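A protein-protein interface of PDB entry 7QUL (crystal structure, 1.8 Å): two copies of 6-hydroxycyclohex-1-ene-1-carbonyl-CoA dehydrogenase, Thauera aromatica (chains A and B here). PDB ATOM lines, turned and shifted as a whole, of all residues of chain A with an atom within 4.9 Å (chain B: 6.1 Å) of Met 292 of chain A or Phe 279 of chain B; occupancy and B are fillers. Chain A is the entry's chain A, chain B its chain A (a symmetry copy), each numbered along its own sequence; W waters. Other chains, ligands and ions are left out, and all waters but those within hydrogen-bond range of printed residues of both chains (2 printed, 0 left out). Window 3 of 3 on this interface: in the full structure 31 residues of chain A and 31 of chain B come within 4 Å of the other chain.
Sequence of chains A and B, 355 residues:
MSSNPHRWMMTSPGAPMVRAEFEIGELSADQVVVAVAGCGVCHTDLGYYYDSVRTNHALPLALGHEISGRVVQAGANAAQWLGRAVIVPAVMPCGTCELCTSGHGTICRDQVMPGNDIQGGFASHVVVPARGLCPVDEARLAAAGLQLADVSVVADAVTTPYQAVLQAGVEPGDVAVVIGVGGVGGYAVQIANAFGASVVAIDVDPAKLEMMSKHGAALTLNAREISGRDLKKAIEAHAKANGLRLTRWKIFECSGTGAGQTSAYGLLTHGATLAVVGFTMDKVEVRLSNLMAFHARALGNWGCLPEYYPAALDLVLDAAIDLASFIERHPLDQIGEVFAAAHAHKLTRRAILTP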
ATOM      1  N   LEU A 288     -23.116  10.514  20.425  1.00  0.00           N
ATOM      2  CA  LEU A 288     -23.909  11.095  21.534  1.00  0.00           C
ATOM      3  C   LEU A 288     -23.981  10.085  22.688  1.00  0.00           C
ATOM      4  O   LEU A 288     -24.070  10.535  23.833  1.00  0.00           O
ATOM      5  CB  LEU A 288     -25.291  11.483  20.999  1.00  0.00           C
ATOM      6  N   SER A 289     -23.886   8.777  22.425  1.00  0.00           N
ATOM      7  CA  SER A 289     -24.112   7.720  23.447  1.00  0.00           C
ATOM      8  C   SER A 289     -22.922   7.593  24.396  1.00  0.00           C
ATOM      9  O   SER A 289     -23.101   6.955  25.447  1.00  0.00           O
ATOM     10  CB  SER A 289     -24.473   6.404  22.806  1.00  0.00           C
ATOM     11  OG  SER A 289     -25.764   6.526  22.217  1.00  0.00           O
ATOM     12  N   ASN A 290     -21.767   8.182  24.075  1.00  0.00           N
ATOM     13  CA  ASN A 290     -20.647   8.295  25.040  1.00  0.00           C
ATOM     14  C   ASN A 290     -21.149   8.975  26.323  1.00  0.00           C
ATOM     15  O   ASN A 290     -20.724   8.555  27.397  1.00  0.00           O
ATOM     16  CB  ASN A 290     -19.424   8.970  24.423  1.00  0.00           C
ATOM     17  CG  ASN A 290     -18.756   8.079  23.400  1.00  0.00           C
ATOM     18  OD1 ASN A 290     -19.348   7.090  22.965  1.00  0.00           O
ATOM     19  ND2 ASN A 290     -17.527   8.405  23.041  1.00  0.00           N
ATOM     20  N   LEU A 291     -22.054   9.938  26.206  1.00  0.00           N
ATOM     21  CA  LEU A 291     -22.687  10.648  27.358  1.00  0.00           C
ATOM     22  C   LEU A 291     -23.340   9.619  28.283  1.00  0.00           C
ATOM     23  O   LEU A 291     -23.293   9.786  29.516  1.00  0.00           O
ATOM     24  CB  LEU A 291     -23.725  11.651  26.835  1.00  0.00           C
ATOM     25  CG  LEU A 291     -23.316  13.129  26.770  1.00  0.00           C
ATOM     26  CD1 LEU A 291     -21.819  13.362  26.663  1.00  0.00           C
ATOM     27  CD2 LEU A 291     -24.034  13.838  25.636  1.00  0.00           C
ATOM     28  N   MET A 292     -23.926   8.579  27.704  1.00  0.00           N
ATOM     29  CA  MET A 292     -24.576   7.498  28.483  1.00  0.00           C
ATOM     30  C   MET A 292     -23.528   6.677  29.220  1.00  0.00           C
ATOM     31  O   MET A 292     -23.639   6.590  30.452  1.00  0.00           O
ATOM     32  CB  MET A 292     -25.376   6.590  27.566  1.00  0.00           C
ATOM     33  CG  MET A 292     -26.436   7.334  26.811  1.00  0.00           C
ATOM     34  SD  MET A 292     -27.218   6.274  25.598  1.00  0.00           S
ATOM     35  CE  MET A 292     -27.497   4.858  26.675  1.00  0.00           C
ATOM     36  N   ALA A 293     -22.560   6.091  28.506  1.00  0.00           N
ATOM     37  CA  ALA A 293     -21.538   5.191  29.096  1.00  0.00           C
ATOM     38  C   ALA A 293     -20.821   5.872  30.264  1.00  0.00           C
ATOM     39  O   ALA A 293     -20.375   5.147  31.171  1.00  0.00           O
ATOM     40  CB  ALA A 293     -20.530   4.768  28.062  1.00  0.00           C
ATOM     41  N   PHE A 294     -20.681   7.197  30.220  1.00  0.00           N
ATOM     42  CA  PHE A 294     -19.901   7.962  31.216  1.00  0.00           C
ATOM     43  C   PHE A 294     -20.847   8.589  32.248  1.00  0.00           C
ATOM     44  O   PHE A 294     -20.343   9.203  33.200  1.00  0.00           O
ATOM     45  CB  PHE A 294     -19.006   8.967  30.496  1.00  0.00           C
ATOM     46  CG  PHE A 294     -17.788   8.357  29.847  1.00  0.00           C
ATOM     47  CD1 PHE A 294     -16.899   7.600  30.594  1.00  0.00           C
ATOM     48  CD2 PHE A 294     -17.538   8.528  28.494  1.00  0.00           C
ATOM     49  CE1 PHE A 294     -15.790   7.008  30.003  1.00  0.00           C
ATOM     50  CE2 PHE A 294     -16.433   7.938  27.900  1.00  0.00           C
ATOM     51  CZ  PHE A 294     -15.558   7.182  28.654  1.00  0.00           C
ATOM     52  N   HIS A 295     -22.149   8.381  32.106  1.00  0.00           N
ATOM     53  CA  HIS A 295     -23.226   9.135  32.815  1.00  0.00           C
ATOM     54  C   HIS A 295     -22.824  10.620  32.906  1.00  0.00           C
ATOM     55  O   HIS A 295     -22.710  11.169  34.011  1.00  0.00           O
ATOM     56  CB  HIS A 295     -23.525   8.497  34.176  1.00  0.00           C
ATOM     57  CG  HIS A 295     -24.745   9.055  34.813  1.00  0.00           C
ATOM     58  ND1 HIS A 295     -24.693   9.849  35.946  1.00  0.00           N
ATOM     59  CD2 HIS A 295     -26.049   8.933  34.486  1.00  0.00           C
ATOM     60  CE1 HIS A 295     -25.924  10.193  36.281  1.00  0.00           C
ATOM     61  NE2 HIS A 295     -26.771   9.650  35.403  1.00  0.00           N
ATOM     62  N   ILE B 107     -22.741   4.238  36.893  1.00  0.00           N
ATOM     63  CA  ILE B 107     -21.430   4.025  36.198  1.00  0.00           C
ATOM     64  C   ILE B 107     -20.443   3.199  37.050  1.00  0.00           C
ATOM     65  O   ILE B 107     -19.354   2.915  36.497  1.00  0.00           O
ATOM     66  CB  ILE B 107     -20.800   5.357  35.722  1.00  0.00           C
ATOM     67  CG1 ILE B 107     -20.925   6.528  36.702  1.00  0.00           C
ATOM     68  CG2 ILE B 107     -21.391   5.717  34.367  1.00  0.00           C
ATOM     69  CD1 ILE B 107     -20.262   6.335  38.052  1.00  0.00           C
ATOM     70  N   GLU B 253     -34.333  11.175  23.618  1.00  0.00           N
ATOM     71  CA  GLU B 253     -33.995  10.333  22.453  1.00  0.00           C
ATOM     72  C   GLU B 253     -33.980   8.890  22.962  1.00  0.00           C
ATOM     73  O   GLU B 253     -33.059   8.530  23.715  1.00  0.00           O
ATOM     74  CB  GLU B 253     -32.693  10.807  21.829  1.00  0.00           C
ATOM     75  CG  GLU B 253     -32.520  10.345  20.393  1.00  0.00           C
ATOM     76  CD  GLU B 253     -32.890   8.894  20.129  1.00  0.00           C
ATOM     77  OE1 GLU B 253     -33.889   8.677  19.454  1.00  0.00           O
ATOM     78  OE2 GLU B 253     -32.190   7.993  20.622  1.00  0.00           O
ATOM     79  N   CYS B 254     -34.977   8.107  22.553  1.00  0.00           N
ATOM     80  CA  CYS B 254     -35.227   6.751  23.096  1.00  0.00           C
ATOM     81  C   CYS B 254     -35.090   5.707  21.988  1.00  0.00           C
ATOM     82  O   CYS B 254     -35.033   4.501  22.327  1.00  0.00           O
ATOM     83  CB  CYS B 254     -36.592   6.673  23.754  1.00  0.00           C
ATOM     84  SG  CYS B 254     -36.667   7.595  25.315  1.00  0.00           S
ATOM     85  N   SER B 255     -34.948   6.120  20.723  1.00  0.00           N
ATOM     86  CA  SER B 255     -34.842   5.155  19.598  1.00  0.00           C
ATOM     87  C   SER B 255     -33.470   4.479  19.593  1.00  0.00           C
ATOM     88  O   SER B 255     -33.393   3.340  19.103  1.00  0.00           O
ATOM     89  CB  SER B 255     -35.134   5.795  18.268  1.00  0.00           C
ATOM     90  OG  SER B 255     -34.044   6.580  17.853  1.00  0.00           O
ATOM     91  N   GLY B 256     -32.424   5.169  20.049  1.00  0.00           N
ATOM     92  CA  GLY B 256     -31.036   4.696  19.936  1.00  0.00           C
ATOM     93  C   GLY B 256     -30.669   4.491  18.478  1.00  0.00           C
ATOM     94  O   GLY B 256     -30.209   3.396  18.109  1.00  0.00           O
ATOM     95  N   THR B 257     -30.958   5.490  17.661  1.00  0.00           N
ATOM     96  CA  THR B 257     -30.541   5.575  16.238  1.00  0.00           C
ATOM     97  C   THR B 257     -29.933   6.950  16.019  1.00  0.00           C
ATOM     98  O   THR B 257     -30.432   7.882  16.637  1.00  0.00           O
ATOM     99  CB  THR B 257     -31.747   5.348  15.307  1.00  0.00           C
ATOM    100  OG1 THR B 257     -32.795   6.293  15.556  1.00  0.00           O
ATOM    101  CG2 THR B 257     -32.326   3.961  15.465  1.00  0.00           C
ATOM    102  N   GLN B 261     -31.510  10.667  17.044  1.00  0.00           N
ATOM    103  CA  GLN B 261     -30.565  11.629  17.691  1.00  0.00           C
ATOM    104  C   GLN B 261     -30.494  12.937  16.888  1.00  0.00           C
ATOM    105  O   GLN B 261     -30.646  14.008  17.476  1.00  0.00           O
ATOM    106  CB  GLN B 261     -29.177  11.026  17.835  1.00  0.00           C
ATOM    107  CG  GLN B 261     -29.088   9.954  18.913  1.00  0.00           C
ATOM    108  CD  GLN B 261     -27.742   9.277  18.950  1.00  0.00           C
ATOM    109  OE1 GLN B 261     -26.928   9.371  18.032  1.00  0.00           O
ATOM    110  NE2 GLN B 261     -27.486   8.567  20.030  1.00  0.00           N
ATOM    111  N   VAL B 276     -30.402  11.654  26.588  1.00  0.00           N
ATOM    112  CA  VAL B 276     -29.856  10.577  25.728  1.00  0.00           C
ATOM    113  C   VAL B 276     -30.051   9.260  26.473  1.00  0.00           C
ATOM    114  O   VAL B 276     -29.371   8.999  27.494  1.00  0.00           O
ATOM    115  CB  VAL B 276     -28.395  10.883  25.363  1.00  0.00           C
ATOM    116  CG1 VAL B 276     -27.851   9.903  24.321  1.00  0.00           C
ATOM    117  CG2 VAL B 276     -28.241  12.321  24.902  1.00  0.00           C
ATOM    118  N   VAL B 277     -31.059   8.507  26.044  1.00  0.00           N
ATOM    119  CA  VAL B 277     -31.565   7.296  26.740  1.00  0.00           C
ATOM    120  C   VAL B 277     -31.257   6.057  25.882  1.00  0.00           C
ATOM    121  O   VAL B 277     -30.870   5.042  26.450  1.00  0.00           O
ATOM    122  CB  VAL B 277     -33.064   7.462  27.073  1.00  0.00           C
ATOM    123  CG1 VAL B 277     -33.572   6.366  28.000  1.00  0.00           C
ATOM    124  CG2 VAL B 277     -33.368   8.834  27.666  1.00  0.00           C
ATOM    125  N   GLY B 278     -31.385   6.146  24.560  1.00  0.00           N
ATOM    126  CA  GLY B 278     -31.164   5.017  23.635  1.00  0.00           C
ATOM    127  C   GLY B 278     -29.700   4.858  23.270  1.00  0.00           C
ATOM    128  O   GLY B 278     -29.059   5.830  22.857  1.00  0.00           O
ATOM    129  N   PHE B 279     -29.148   3.663  23.426  1.00  0.00           N
ATOM    130  CA  PHE B 279     -27.715   3.443  23.132  1.00  0.00           C
ATOM    131  C   PHE B 279     -27.587   3.049  21.658  1.00  0.00           C
ATOM    132  O   PHE B 279     -28.348   2.200  21.195  1.00  0.00           O
ATOM    133  CB  PHE B 279     -27.076   2.382  24.021  1.00  0.00           C
ATOM    134  CG  PHE B 279     -25.611   2.221  23.715  1.00  0.00           C
ATOM    135  CD1 PHE B 279     -24.671   3.061  24.297  1.00  0.00           C
ATOM    136  CD2 PHE B 279     -25.184   1.336  22.743  1.00  0.00           C
ATOM    137  CE1 PHE B 279     -23.321   2.952  23.984  1.00  0.00           C
ATOM    138  CE2 PHE B 279     -23.837   1.249  22.407  1.00  0.00           C
ATOM    139  CZ  PHE B 279     -22.907   2.054  23.024  1.00  0.00           C
ATOM    140  N   THR B 280     -26.628   3.652  20.968  1.00  0.00           N
ATOM    141  CA  THR B 280     -26.131   3.195  19.646  1.00  0.00           C
ATOM    142  C   THR B 280     -24.685   3.651  19.505  1.00  0.00           C
ATOM    143  O   THR B 280     -24.321   4.712  20.085  1.00  0.00           O
ATOM    144  CB  THR B 280     -27.036   3.691  18.510  1.00  0.00           C
ATOM    145  OG1 THR B 280     -26.519   3.272  17.246  1.00  0.00           O
ATOM    146  CG2 THR B 280     -27.182   5.199  18.507  1.00  0.00           C
ATOM    147  N   MET B 281     -23.882   2.866  18.783  1.00  0.00           N
ATOM    148  CA  MET B 281     -22.472   3.212  18.470  1.00  0.00           C
ATOM    149  C   MET B 281     -22.398   4.166  17.270  1.00  0.00           C
ATOM    150  O   MET B 281     -21.287   4.635  16.976  1.00  0.00           O
ATOM    151  CB  MET B 281     -21.652   1.953  18.180  1.00  0.00           C
ATOM    152  CG  MET B 281     -21.372   1.168  19.431  1.00  0.00           C
ATOM    153  SD  MET B 281     -20.278   2.104  20.540  1.00  0.00           S
ATOM    154  CE  MET B 281     -18.694   1.858  19.733  1.00  0.00           C
ATOM    155  N   GLY B 300     -26.723  12.346  29.604  1.00  0.00           N
ATOM    156  CA  GLY B 300     -26.587  10.908  29.318  1.00  0.00           C
ATOM    157  C   GLY B 300     -27.135  10.053  30.447  1.00  0.00           C
ATOM    158  O   GLY B 300     -26.655  10.185  31.572  1.00  0.00           O
ATOM    159  N   ASN B 301     -28.070   9.156  30.146  1.00  0.00           N
ATOM    160  CA  ASN B 301     -28.641   8.197  31.119  1.00  0.00           C
ATOM    161  C   ASN B 301     -27.977   6.833  30.920  1.00  0.00           C
ATOM    162  O   ASN B 301     -27.928   6.355  29.771  1.00  0.00           O
ATOM    163  CB  ASN B 301     -30.161   8.060  30.950  1.00  0.00           C
ATOM    164  CG  ASN B 301     -30.791   7.521  32.206  1.00  0.00           C
ATOM    165  OD1 ASN B 301     -30.694   8.159  33.245  1.00  0.00           O
ATOM    166  ND2 ASN B 301     -31.368   6.333  32.155  1.00  0.00           N
ATOM    167  N   TRP B 302     -27.516   6.222  32.001  1.00  0.00           N
ATOM    168  CA  TRP B 302     -27.151   4.784  32.061  1.00  0.00           C
ATOM    169  C   TRP B 302     -28.018   4.052  33.095  1.00  0.00           C
ATOM    170  O   TRP B 302     -27.842   4.269  34.320  1.00  0.00           O
ATOM    171  CB  TRP B 302     -25.666   4.644  32.384  1.00  0.00           C
ATOM    172  CG  TRP B 302     -25.131   3.274  32.138  1.00  0.00           C
ATOM    173  CD1 TRP B 302     -24.841   2.321  33.068  1.00  0.00           C
ATOM    174  CD2 TRP B 302     -24.810   2.703  30.854  1.00  0.00           C
ATOM    175  NE1 TRP B 302     -24.381   1.191  32.450  1.00  0.00           N
ATOM    176  CE2 TRP B 302     -24.351   1.393  31.093  1.00  0.00           C
ATOM    177  CE3 TRP B 302     -24.874   3.171  29.535  1.00  0.00           C
ATOM    178  CZ2 TRP B 302     -23.938   0.551  30.058  1.00  0.00           C
ATOM    179  CZ3 TRP B 302     -24.476   2.336  28.512  1.00  0.00           C
ATOM    180  CH2 TRP B 302     -24.014   1.041  28.774  1.00  0.00           C
HETATM  181  O   HOH W   1     -24.352   9.699  18.039  1.00  0.00           O
HETATM  182  O   HOH W   2     -24.586   7.400  19.945  1.00  0.00           O
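OG of Ser 289 of chain A is in hydrogen-bond range of O of Thr 280 of chain B, 3.1 Å away. NE2 of Gln 261 of chain B sits at hydrogen-bond distance from OG of Ser 289 of chain A, at 3.5 Å. OG of Ser 289 of chain A is in hydrogen-bond range of O of Gly 278 of chain B (3.4 Å). The side-chain sulfur (SD) of Met 292 of chain A sits close to the backbone carbonyl oxygen (O) of Gly 278 of chain B, 3.3 Å away.
O of Glu 253 of chain B sits at hydrogen-bond distance from N of Val 277 of chain B, 3.1 Å away. The backbone NH (N) of Gly 278 of chain B sits at hydrogen-bond distance from the backbone carbonyl oxygen (O) of Glu 253 of chain B (3.0 Å). The side-chain hydroxyl (OG) of Ser 289 of chain A is in hydrogen-bond range of the side-chain sulfur (SD) of Met 292 of chain A, at 3.7 Å. The backbone carbonyl oxygen (O) of Val 276 of chain B sits at hydrogen-bond distance from the backbone NH (N) of Asn 301 of chain B.
Among the printed residues, pairs that only touch across the chains: Leu 288 of chain A with Gln 261 of chain B (3.8 Å), Leu 288 of chain A with Val 276 of chain B (3.9 Å), Ser 289 of chain A with Phe 279 of chain B (3.7 Å), Leu 291 of chain A with Gly 300 of chain B (3.5 Å), Met 292 of chain A with Val 276 of chain B (3.4 Å), Met 292 of chain A with Val 277 of chain B (3.4 Å), Met 292 of chain A with Phe 279 of chain B (3.7 Å), Met 292 of chain A with Gly 300 of chain B (3.9 Å), Met 292 of chain A with Asn 301 of chain B (3.4 Å), Met 292 of chain A with Trp 302 of chain B (3.4 Å), Ala 293 of chain A with Ile 107 of chain B (3.4 Å), Ala 293 of chain A with Trp 302 of chain B (3.9 Å), Phe 294 of chain A with Ile 107 of chain B (3.6 Å), His 295 of chain A with Ile 107 of chain B (3.5 Å), His 295 of chain A with Gly 300 of chain B (3.2 Å) and His 295 of chain A with Trp 302 of chain B (3.96 Å).
Printed residues of chain B within 4 Å of Met 292 of chain A: Val 276 (3.4 Å), Val 277 (3.4 Å), Gly 278 (3.3 Å), Phe 279 (3.7 Å), Gly 300 (3.9 Å), Asn 301 (3.4 Å) and Trp 302 (3.4 Å). Of chain A, only Ser 289 (3.7 Å) and Met 292 (3.7 Å) come within 4 Å of Phe 279 of chain B. Printed residues of chain A within 4 Å of Gly 278 of chain B: Ser 289 and Met 292. Printed residues of chain B within 4 Å of Ser 289 of chain A: Gln 261 (3.5 Å), Gly 278 (3.4 Å), Phe 279 (3.7 Å) and Thr 280 (3.1 Å). Of the printed residues of chain B, His 295 of chain A touches Ile 107, Gly 300 and Trp 302. Asn 290 of chain A touches none of the printed residues of chain B. The nearest residue of chain B that does not touch Met 292 of chain A is Ile 107 of chain B (4.6 Å). The nearest printed residue of chain B that does not touch Ser 289 of chain A is Val 276 of chain B (4.4 Å).
Along chain B the printed residues that touch a printed residue of chain A span positions 107 to 302. Of the 8 printed residues of chain A, 7 touch a printed residue of chain B. Printed residues of chain A that touch a printed residue of chain B: Leu 288, Ser 289, Leu 291, Met 292, Ala 293, Phe 294 and His 295. Among the printed residues, 20 pairs touch across the chains.
No position is printed for both chains.
Water W1 bridges OE1 of Gln 261 of chain B (2.6 Å) and N of Leu 288 of chain A (2.8 Å). Water W2 lies within hydrogen-bond range of the side-chain hydroxyl of Ser 289 of chain A, the backbone carbonyl oxygen of Thr 280 of chain B, the side-chain amide nitrogen of Gln 261 of chain B and the backbone NH of Leu 288 of chain A.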
